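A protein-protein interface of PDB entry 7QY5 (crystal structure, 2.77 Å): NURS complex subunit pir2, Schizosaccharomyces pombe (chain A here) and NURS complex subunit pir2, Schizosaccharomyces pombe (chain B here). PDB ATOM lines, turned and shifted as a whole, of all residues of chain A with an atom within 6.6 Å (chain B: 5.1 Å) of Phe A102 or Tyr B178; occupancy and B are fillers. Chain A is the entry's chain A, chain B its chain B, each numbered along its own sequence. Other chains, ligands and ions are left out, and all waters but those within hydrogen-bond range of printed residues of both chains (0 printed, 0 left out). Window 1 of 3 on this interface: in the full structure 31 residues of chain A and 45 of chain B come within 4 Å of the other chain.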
ATOM      1  N   ALA A  97      10.991 -24.384  26.839  1.00  0.00           N
ATOM      2  CA  ALA A  97      11.623 -25.657  26.412  1.00  0.00           C
ATOM      3  C   ALA A  97      10.612 -26.506  25.630  1.00  0.00           C
ATOM      4  O   ALA A  97      11.019 -27.141  24.630  1.00  0.00           O
ATOM      5  CB  ALA A  97      12.165 -26.398  27.602  1.00  0.00           C
ATOM      6  N   LEU A  98       9.347 -26.510  26.072  1.00  0.00           N
ATOM      7  CA  LEU A  98       8.192 -27.145  25.365  1.00  0.00           C
ATOM      8  C   LEU A  98       7.957 -26.500  23.987  1.00  0.00           C
ATOM      9  O   LEU A  98       7.621 -27.247  23.030  1.00  0.00           O
ATOM     10  CB  LEU A  98       6.933 -26.992  26.222  1.00  0.00           C
ATOM     11  CG  LEU A  98       6.863 -27.852  27.478  1.00  0.00           C
ATOM     12  CD1 LEU A  98       5.645 -27.447  28.292  1.00  0.00           C
ATOM     13  CD2 LEU A  98       6.815 -29.342  27.140  1.00  0.00           C
ATOM     14  N   TYR A  99       8.073 -25.171  23.902  1.00  0.00           N
ATOM     15  CA  TYR A  99       8.081 -24.420  22.620  1.00  0.00           C
ATOM     16  C   TYR A  99       9.177 -24.994  21.707  1.00  0.00           C
ATOM     17  O   TYR A  99       8.857 -25.401  20.558  1.00  0.00           O
ATOM     18  CB  TYR A  99       8.259 -22.918  22.879  1.00  0.00           C
ATOM     19  CG  TYR A  99       8.332 -22.069  21.637  1.00  0.00           C
ATOM     20  CD1 TYR A  99       9.439 -22.118  20.812  1.00  0.00           C
ATOM     21  CD2 TYR A  99       7.300 -21.222  21.282  1.00  0.00           C
ATOM     22  CE1 TYR A  99       9.514 -21.368  19.650  1.00  0.00           C
ATOM     23  CE2 TYR A  99       7.362 -20.453  20.126  1.00  0.00           C
ATOM     24  CZ  TYR A  99       8.473 -20.527  19.298  1.00  0.00           C
ATOM     25  OH  TYR A  99       8.574 -19.782  18.151  1.00  0.00           O
ATOM     26  N   ASP A 100      10.426 -25.028  22.205  1.00  0.00           N
ATOM     27  CA  ASP A 100      11.654 -25.298  21.402  1.00  0.00           C
ATOM     28  C   ASP A 100      11.623 -26.739  20.889  1.00  0.00           C
ATOM     29  O   ASP A 100      12.030 -26.973  19.737  1.00  0.00           O
ATOM     30  CB  ASP A 100      12.923 -25.021  22.203  1.00  0.00           C
ATOM     31  CG  ASP A 100      13.119 -23.563  22.570  1.00  0.00           C
ATOM     32  OD1 ASP A 100      12.199 -22.778  22.326  1.00  0.00           O
ATOM     33  OD2 ASP A 100      14.186 -23.229  23.122  1.00  0.00           O
ATOM     34  N   LYS A 101      11.135 -27.662  21.713  1.00  0.00           N
ATOM     35  CA  LYS A 101      10.859 -29.063  21.305  1.00  0.00           C
ATOM     36  C   LYS A 101       9.906 -29.026  20.100  1.00  0.00           C
ATOM     37  O   LYS A 101      10.221 -29.572  19.032  1.00  0.00           O
ATOM     38  CB  LYS A 101      10.295 -29.833  22.506  1.00  0.00           C
ATOM     39  CG  LYS A 101      10.169 -31.339  22.325  1.00  0.00           C
ATOM     40  CD  LYS A 101       9.776 -32.070  23.605  1.00  0.00           C
ATOM     41  CE  LYS A 101       9.914 -33.579  23.497  1.00  0.00           C
ATOM     42  NZ  LYS A 101       9.842 -34.244  24.820  1.00  0.00           N
ATOM     43  N   PHE A 102       8.772 -28.365  20.264  1.00  0.00           N
ATOM     44  CA  PHE A 102       7.713 -28.319  19.231  1.00  0.00           C
ATOM     45  C   PHE A 102       8.323 -27.861  17.901  1.00  0.00           C
ATOM     46  O   PHE A 102       8.188 -28.576  16.881  1.00  0.00           O
ATOM     47  CB  PHE A 102       6.576 -27.402  19.676  1.00  0.00           C
ATOM     48  CG  PHE A 102       5.420 -27.463  18.729  1.00  0.00           C
ATOM     49  CD1 PHE A 102       5.402 -26.658  17.610  1.00  0.00           C
ATOM     50  CD2 PHE A 102       4.405 -28.381  18.914  1.00  0.00           C
ATOM     51  CE1 PHE A 102       4.356 -26.736  16.710  1.00  0.00           C
ATOM     52  CE2 PHE A 102       3.359 -28.458  18.013  1.00  0.00           C
ATOM     53  CZ  PHE A 102       3.337 -27.635  16.914  1.00  0.00           C
ATOM     54  N   MET A 103       8.998 -26.709  17.920  1.00  0.00           N
ATOM     55  CA  MET A 103       9.530 -26.070  16.695  1.00  0.00           C
ATOM     56  C   MET A 103      10.607 -26.957  16.069  1.00  0.00           C
ATOM     57  O   MET A 103      10.552 -27.142  14.837  1.00  0.00           O
ATOM     58  CB  MET A 103      10.071 -24.677  17.005  1.00  0.00           C
ATOM     59  CG  MET A 103       8.949 -23.688  17.276  1.00  0.00           C
ATOM     60  SD  MET A 103       7.579 -23.838  16.075  1.00  0.00           S
ATOM     61  CE  MET A 103       6.251 -23.106  17.021  1.00  0.00           C
ATOM     62  N   ASP A 104      11.497 -27.538  16.880  1.00  0.00           N
ATOM     63  CA  ASP A 104      12.466 -28.565  16.405  1.00  0.00           C
ATOM     64  C   ASP A 104      11.693 -29.710  15.752  1.00  0.00           C
ATOM     65  O   ASP A 104      12.117 -30.167  14.696  1.00  0.00           O
ATOM     66  CB  ASP A 104      13.357 -29.105  17.523  1.00  0.00           C
ATOM     67  CG  ASP A 104      14.418 -28.120  17.975  1.00  0.00           C
ATOM     68  OD1 ASP A 104      14.643 -27.116  17.269  1.00  0.00           O
ATOM     69  OD2 ASP A 104      15.002 -28.353  19.041  1.00  0.00           O
ATOM     70  N   ARG A 105      10.599 -30.147  16.361  1.00  0.00           N
ATOM     71  CA  ARG A 105       9.756 -31.230  15.806  1.00  0.00           C
ATOM     72  C   ARG A 105       9.088 -30.720  14.527  1.00  0.00           C
ATOM     73  O   ARG A 105       8.996 -31.485  13.542  1.00  0.00           O
ATOM     74  CB  ARG A 105       8.729 -31.686  16.842  1.00  0.00           C
ATOM     75  CG  ARG A 105       9.302 -32.577  17.926  1.00  0.00           C
ATOM     76  CD  ARG A 105       8.276 -32.917  18.984  1.00  0.00           C
ATOM     77  NE  ARG A 105       8.563 -34.212  19.573  1.00  0.00           N
ATOM     78  CZ  ARG A 105       7.851 -34.771  20.531  1.00  0.00           C
ATOM     79  NH1 ARG A 105       6.803 -34.149  21.026  1.00  0.00           N
ATOM     80  NH2 ARG A 105       8.183 -35.960  20.993  1.00  0.00           N
ATOM     81  N   LEU A 106       8.608 -29.482  14.533  1.00  0.00           N
ATOM     82  CA  LEU A 106       7.904 -28.942  13.346  1.00  0.00           C
ATOM     83  C   LEU A 106       8.841 -29.081  12.154  1.00  0.00           C
ATOM     84  O   LEU A 106       8.409 -29.689  11.148  1.00  0.00           O
ATOM     85  CB  LEU A 106       7.543 -27.472  13.557  1.00  0.00           C
ATOM     86  CG  LEU A 106       6.924 -26.767  12.352  1.00  0.00           C
ATOM     87  CD1 LEU A 106       5.650 -27.475  11.893  1.00  0.00           C
ATOM     88  CD2 LEU A 106       6.643 -25.310  12.688  1.00  0.00           C
ATOM     89  N   ASP A 107      10.066 -28.569  12.328  1.00  0.00           N
ATOM     90  CA  ASP A 107      11.105 -28.404  11.285  1.00  0.00           C
ATOM     91  C   ASP A 107      11.639 -29.761  10.826  1.00  0.00           C
ATOM     92  O   ASP A 107      12.003 -29.864   9.656  1.00  0.00           O
ATOM     93  CB  ASP A 107      12.263 -27.561  11.805  1.00  0.00           C
ATOM     94  CG  ASP A 107      11.848 -26.160  12.204  1.00  0.00           C
ATOM     95  OD1 ASP A 107      11.001 -25.559  11.493  1.00  0.00           O
ATOM     96  OD2 ASP A 107      12.377 -25.683  13.222  1.00  0.00           O
ATOM     97  N   TYR A 110       8.037 -33.706  11.853  1.00  0.00           N
ATOM     98  CA  TYR A 110       7.285 -34.503  12.858  1.00  0.00           C
ATOM     99  C   TYR A 110       5.784 -34.335  12.608  1.00  0.00           C
ATOM    100  O   TYR A 110       5.053 -35.292  12.796  1.00  0.00           O
ATOM    101  CB  TYR A 110       7.711 -34.054  14.261  1.00  0.00           C
ATOM    102  CG  TYR A 110       7.194 -34.835  15.447  1.00  0.00           C
ATOM    103  CD1 TYR A 110       6.018 -34.470  16.079  1.00  0.00           C
ATOM    104  CD2 TYR A 110       7.917 -35.879  15.999  1.00  0.00           C
ATOM    105  CE1 TYR A 110       5.552 -35.150  17.193  1.00  0.00           C
ATOM    106  CE2 TYR A 110       7.457 -36.579  17.105  1.00  0.00           C
ATOM    107  CZ  TYR A 110       6.267 -36.216  17.710  1.00  0.00           C
ATOM    108  OH  TYR A 110       5.795 -36.884  18.811  1.00  0.00           O
ATOM    109  N   TYR A 111       5.350 -33.150  12.172  1.00  0.00           N
ATOM    110  CA  TYR A 111       3.924 -32.736  12.144  1.00  0.00           C
ATOM    111  C   TYR A 111       3.431 -32.559  10.702  1.00  0.00           C
ATOM    112  O   TYR A 111       2.327 -32.004  10.510  1.00  0.00           O
ATOM    113  CB  TYR A 111       3.731 -31.444  12.947  1.00  0.00           C
ATOM    114  CG  TYR A 111       3.869 -31.562  14.451  1.00  0.00           C
ATOM    115  CD1 TYR A 111       3.093 -32.442  15.197  1.00  0.00           C
ATOM    116  CD2 TYR A 111       4.747 -30.746  15.150  1.00  0.00           C
ATOM    117  CE1 TYR A 111       3.208 -32.524  16.580  1.00  0.00           C
ATOM    118  CE2 TYR A 111       4.871 -30.812  16.531  1.00  0.00           C
ATOM    119  CZ  TYR A 111       4.099 -31.703  17.255  1.00  0.00           C
ATOM    120  OH  TYR A 111       4.240 -31.747  18.618  1.00  0.00           O
ATOM    121  N   PHE A 114       0.663 -34.905  10.227  1.00  0.00           N
ATOM    122  CA  PHE A 114      -0.220 -34.797  11.417  1.00  0.00           C
ATOM    123  C   PHE A 114      -1.572 -34.198  11.026  1.00  0.00           C
ATOM    124  O   PHE A 114      -1.640 -33.283  10.177  1.00  0.00           O
ATOM    125  CB  PHE A 114       0.405 -33.963  12.534  1.00  0.00           C
ATOM    126  CG  PHE A 114      -0.528 -33.699  13.685  1.00  0.00           C
ATOM    127  CD1 PHE A 114      -1.221 -32.506  13.769  1.00  0.00           C
ATOM    128  CD2 PHE A 114      -0.748 -34.656  14.664  1.00  0.00           C
ATOM    129  CE1 PHE A 114      -2.095 -32.272  14.822  1.00  0.00           C
ATOM    130  CE2 PHE A 114      -1.616 -34.419  15.717  1.00  0.00           C
ATOM    131  CZ  PHE A 114      -2.293 -33.230  15.792  1.00  0.00           C
ATOM    132  N   ILE B 129      -2.658 -18.523  20.453  1.00  0.00           N
ATOM    133  CA  ILE B 129      -1.194 -18.591  20.190  1.00  0.00           C
ATOM    134  C   ILE B 129      -0.582 -17.287  20.715  1.00  0.00           C
ATOM    135  O   ILE B 129       0.343 -17.365  21.543  1.00  0.00           O
ATOM    136  CB  ILE B 129      -0.925 -18.847  18.693  1.00  0.00           C
ATOM    137  CG1 ILE B 129      -1.296 -20.281  18.311  1.00  0.00           C
ATOM    138  CG2 ILE B 129       0.511 -18.534  18.309  1.00  0.00           C
ATOM    139  CD1 ILE B 129      -1.496 -20.503  16.829  1.00  0.00           C
ATOM    140  N   LEU B 138       6.983 -16.073  25.225  1.00  0.00           N
ATOM    141  CA  LEU B 138       7.552 -16.923  24.136  1.00  0.00           C
ATOM    142  C   LEU B 138       7.738 -16.082  22.877  1.00  0.00           C
ATOM    143  O   LEU B 138       7.286 -14.942  22.815  1.00  0.00           O
ATOM    144  CB  LEU B 138       6.608 -18.091  23.822  1.00  0.00           C
ATOM    145  CG  LEU B 138       6.170 -18.944  25.006  1.00  0.00           C
ATOM    146  CD1 LEU B 138       5.260 -20.076  24.549  1.00  0.00           C
ATOM    147  CD2 LEU B 138       7.375 -19.489  25.767  1.00  0.00           C
ATOM    148  N   ALA B 142       5.289 -18.371  16.163  1.00  0.00           N
ATOM    149  CA  ALA B 142       4.762 -19.756  16.197  1.00  0.00           C
ATOM    150  C   ALA B 142       3.742 -19.951  15.068  1.00  0.00           C
ATOM    151  O   ALA B 142       3.944 -20.838  14.232  1.00  0.00           O
ATOM    152  CB  ALA B 142       4.155 -20.025  17.545  1.00  0.00           C
ATOM    153  N   ILE B 146       4.410 -22.513  11.723  1.00  0.00           N
ATOM    154  CA  ILE B 146       3.489 -23.663  11.488  1.00  0.00           C
ATOM    155  C   ILE B 146       2.896 -23.538  10.080  1.00  0.00           C
ATOM    156  O   ILE B 146       2.881 -24.538   9.345  1.00  0.00           O
ATOM    157  CB  ILE B 146       2.394 -23.728  12.576  1.00  0.00           C
ATOM    158  CG1 ILE B 146       2.949 -24.220  13.914  1.00  0.00           C
ATOM    159  CG2 ILE B 146       1.218 -24.577  12.120  1.00  0.00           C
ATOM    160  CD1 ILE B 146       2.010 -24.029  15.085  1.00  0.00           C
ATOM    161  N   ASP B 173      -5.783 -28.141  13.276  1.00  0.00           N
ATOM    162  CA  ASP B 173      -5.374 -29.325  14.077  1.00  0.00           C
ATOM    163  C   ASP B 173      -3.979 -29.078  14.655  1.00  0.00           C
ATOM    164  O   ASP B 173      -3.749 -29.437  15.800  1.00  0.00           O
ATOM    165  CB  ASP B 173      -5.356 -30.595  13.233  1.00  0.00           C
ATOM    166  CG  ASP B 173      -6.709 -30.999  12.685  1.00  0.00           C
ATOM    167  OD1 ASP B 173      -7.711 -30.618  13.319  1.00  0.00           O
ATOM    168  OD2 ASP B 173      -6.746 -31.699  11.626  1.00  0.00           O
ATOM    169  N   LEU B 174      -3.071 -28.502  13.873  1.00  0.00           N
ATOM    170  CA  LEU B 174      -1.670 -28.269  14.298  1.00  0.00           C
ATOM    171  C   LEU B 174      -1.650 -27.078  15.250  1.00  0.00           C
ATOM    172  O   LEU B 174      -0.975 -27.189  16.287  1.00  0.00           O
ATOM    173  CB  LEU B 174      -0.779 -28.015  13.077  1.00  0.00           C
ATOM    174  CG  LEU B 174       0.728 -27.993  13.351  1.00  0.00           C
ATOM    175  CD1 LEU B 174       1.139 -29.083  14.327  1.00  0.00           C
ATOM    176  CD2 LEU B 174       1.519 -28.146  12.061  1.00  0.00           C
ATOM    177  N   TYR B 175      -2.349 -25.992  14.915  1.00  0.00           N
ATOM    178  CA  TYR B 175      -2.545 -24.835  15.827  1.00  0.00           C
ATOM    179  C   TYR B 175      -3.133 -25.344  17.145  1.00  0.00           C
ATOM    180  O   TYR B 175      -2.697 -24.853  18.203  1.00  0.00           O
ATOM    181  CB  TYR B 175      -3.481 -23.769  15.257  1.00  0.00           C
ATOM    182  CG  TYR B 175      -2.908 -22.808  14.248  1.00  0.00           C
ATOM    183  CD1 TYR B 175      -1.566 -22.806  13.916  1.00  0.00           C
ATOM    184  CD2 TYR B 175      -3.722 -21.854  13.649  1.00  0.00           C
ATOM    185  CE1 TYR B 175      -1.054 -21.895  13.003  1.00  0.00           C
ATOM    186  CE2 TYR B 175      -3.231 -20.946  12.727  1.00  0.00           C
ATOM    187  CZ  TYR B 175      -1.889 -20.971  12.404  1.00  0.00           C
ATOM    188  OH  TYR B 175      -1.370 -20.098  11.504  1.00  0.00           O
ATOM    189  N   ALA B 176      -4.093 -26.277  17.091  1.00  0.00           N
ATOM    190  CA  ALA B 176      -4.723 -26.870  18.295  1.00  0.00           C
ATOM    191  C   ALA B 176      -3.677 -27.692  19.047  1.00  0.00           C
ATOM    192  O   ALA B 176      -3.656 -27.639  20.299  1.00  0.00           O
ATOM    193  CB  ALA B 176      -5.912 -27.720  17.927  1.00  0.00           C
ATOM    194  N   GLU B 177      -2.853 -28.413  18.285  1.00  0.00           N
ATOM    195  CA  GLU B 177      -1.811 -29.347  18.782  1.00  0.00           C
ATOM    196  C   GLU B 177      -0.667 -28.541  19.396  1.00  0.00           C
ATOM    197  O   GLU B 177      -0.115 -28.971  20.434  1.00  0.00           O
ATOM    198  CB  GLU B 177      -1.289 -30.244  17.656  1.00  0.00           C
ATOM    199  CG  GLU B 177      -0.397 -31.374  18.150  1.00  0.00           C
ATOM    200  CD  GLU B 177      -1.066 -32.345  19.106  1.00  0.00           C
ATOM    201  OE1 GLU B 177      -0.352 -33.134  19.759  1.00  0.00           O
ATOM    202  OE2 GLU B 177      -2.298 -32.313  19.195  1.00  0.00           O
ATOM    203  N   TYR B 178      -0.309 -27.418  18.778  1.00  0.00           N
ATOM    204  CA  TYR B 178       0.690 -26.488  19.353  1.00  0.00           C
ATOM    205  C   TYR B 178       0.282 -26.187  20.800  1.00  0.00           C
ATOM    206  O   TYR B 178       0.997 -26.521  21.747  1.00  0.00           O
ATOM    207  CB  TYR B 178       0.803 -25.213  18.521  1.00  0.00           C
ATOM    208  CG  TYR B 178       1.646 -24.170  19.199  1.00  0.00           C
ATOM    209  CD1 TYR B 178       1.059 -23.130  19.890  1.00  0.00           C
ATOM    210  CD2 TYR B 178       3.031 -24.264  19.208  1.00  0.00           C
ATOM    211  CE1 TYR B 178       1.828 -22.175  20.530  1.00  0.00           C
ATOM    212  CE2 TYR B 178       3.814 -23.321  19.850  1.00  0.00           C
ATOM    213  CZ  TYR B 178       3.206 -22.276  20.517  1.00  0.00           C
ATOM    214  OH  TYR B 178       3.951 -21.342  21.159  1.00  0.00           O
ATOM    215  N   LEU B 179      -0.908 -25.622  20.945  1.00  0.00           N
ATOM    216  CA  LEU B 179      -1.496 -25.236  22.246  1.00  0.00           C
ATOM    217  C   LEU B 179      -1.428 -26.427  23.204  1.00  0.00           C
ATOM    218  O   LEU B 179      -0.999 -26.215  24.350  1.00  0.00           O
ATOM    219  CB  LEU B 179      -2.935 -24.772  22.006  1.00  0.00           C
ATOM    220  CG  LEU B 179      -3.076 -23.477  21.205  1.00  0.00           C
ATOM    221  CD1 LEU B 179      -4.530 -23.210  20.819  1.00  0.00           C
ATOM    222  CD2 LEU B 179      -2.494 -22.305  21.984  1.00  0.00           C
ATOM    223  N   ARG B 180      -1.813 -27.627  22.759  1.00  0.00           N
ATOM    224  CA  ARG B 180      -1.764 -28.855  23.606  1.00  0.00           C
ATOM    225  C   ARG B 180      -0.344 -29.048  24.143  1.00  0.00           C
ATOM    226  O   ARG B 180      -0.193 -29.118  25.359  1.00  0.00           O
ATOM    227  CB  ARG B 180      -2.244 -30.105  22.864  1.00  0.00           C
ATOM    228  CG  ARG B 180      -3.760 -30.210  22.809  1.00  0.00           C
ATOM    229  CD  ARG B 180      -4.237 -31.381  21.985  1.00  0.00           C
ATOM    230  NE  ARG B 180      -4.077 -32.646  22.690  1.00  0.00           N
ATOM    231  CZ  ARG B 180      -4.939 -33.129  23.580  1.00  0.00           C
ATOM    232  NH1 ARG B 180      -6.029 -32.445  23.903  1.00  0.00           N
ATOM    233  NH2 ARG B 180      -4.704 -34.296  24.153  1.00  0.00           N
ATOM    234  N   GLN B 181       0.660 -29.051  23.269  1.00  0.00           N
ATOM    235  CA  GLN B 181       2.053 -29.423  23.617  1.00  0.00           C
ATOM    236  C   GLN B 181       2.770 -28.300  24.374  1.00  0.00           C
ATOM    237  O   GLN B 181       3.641 -28.618  25.188  1.00  0.00           O
ATOM    238  CB  GLN B 181       2.793 -29.794  22.339  1.00  0.00           C
ATOM    239  CG  GLN B 181       2.166 -30.993  21.646  1.00  0.00           C
ATOM    240  CD  GLN B 181       2.085 -32.201  22.547  1.00  0.00           C
ATOM    241  OE1 GLN B 181       2.858 -32.340  23.491  1.00  0.00           O
ATOM    242  NE2 GLN B 181       1.151 -33.094  22.259  1.00  0.00           N
ATOM    243  N   VAL B 182       2.440 -27.037  24.119  1.00  0.00           N
ATOM    244  CA  VAL B 182       3.312 -25.888  24.499  1.00  0.00           C
ATOM    245  C   VAL B 182       2.627 -25.068  25.586  1.00  0.00           C
ATOM    246  O   VAL B 182       3.208 -24.912  26.669  1.00  0.00           O
ATOM    247  CB  VAL B 182       3.634 -25.011  23.280  1.00  0.00           C
ATOM    248  CG1 VAL B 182       4.429 -23.776  23.668  1.00  0.00           C
ATOM    249  CG2 VAL B 182       4.351 -25.810  22.207  1.00  0.00           C
ATOM    250  N   ALA B 183       1.454 -24.528  25.282  1.00  0.00           N
ATOM    251  CA  ALA B 183       0.668 -23.692  26.213  1.00  0.00           C
ATOM    252  C   ALA B 183      -0.248 -24.577  27.061  1.00  0.00           C
ATOM    253  O   ALA B 183      -1.046 -23.998  27.800  1.00  0.00           O
ATOM    254  CB  ALA B 183      -0.132 -22.678  25.437  1.00  0.00           C
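Along chain A the printed residues that touch a printed residue of chain B span positions 98 to 114. Of the 15 printed residues of chain B, 8 touch a printed residue of chain A. Hydrophobic or aromatic side chains of chain B within 4 Å of the printed part of chain A: Ala B142, Ile B146, Leu B174, Tyr B178 and Val B182. Among the printed residues, 15 pairs touch across the chains. Among the printed residues, no Asp or Glu carboxylate lies within 4 Å of a Lys or Arg side-chain nitrogen of the other chain.
Among the printed residues, merely in contact across the chains: Leu A98 with Gln B181 (3.8 Å), Leu A98 with Val B182 (3.7 Å), Tyr A99 with Tyr B178 (3.4 Å), Tyr A99 with Val B182 (3.9 Å), Phe A102 with Ile B146 (3.9 Å), Phe A102 with Leu B174 (3.7 Å), Phe A102 with Tyr B178 (3.6 Å), Phe A102 with Val B182 (3.7 Å), Met A103 with Ala B142 (3.8 Å), Met A103 with Tyr B178 (3.7 Å), Leu A106 with Ile B146 (3.7 Å), Tyr A111 with Leu B174 (3.7 Å), Tyr A111 with Gln B181 (3.7 Å), Phe A114 with Asp B173 (3.4 Å) and Phe A114 with Glu B177 (3.5 Å).
Phe A102 touches four residues of chain B. Of the printed residues of chain A, Tyr B178 touches Tyr A99, Phe A102 and Met A103. Printed residues of chain A within 4 Å of Val B182: Leu A98, Tyr A99 and Phe A102. Of the printed residues of chain A, Leu B174 touches Phe A102 and Tyr A111. Printed residues of chain B within 4 Å of Tyr A111: Leu B174 and Gln B181. Tyr A110 touches none of the printed residues of chain B.
OE2 of Glu B177 lies within salt-bridge range of NE of Arg B180. The side-chain carboxylate (OE1) of Glu B177 sits at hydrogen-bond distance from the side-chain amide nitrogen (NE2) of Gln B181.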
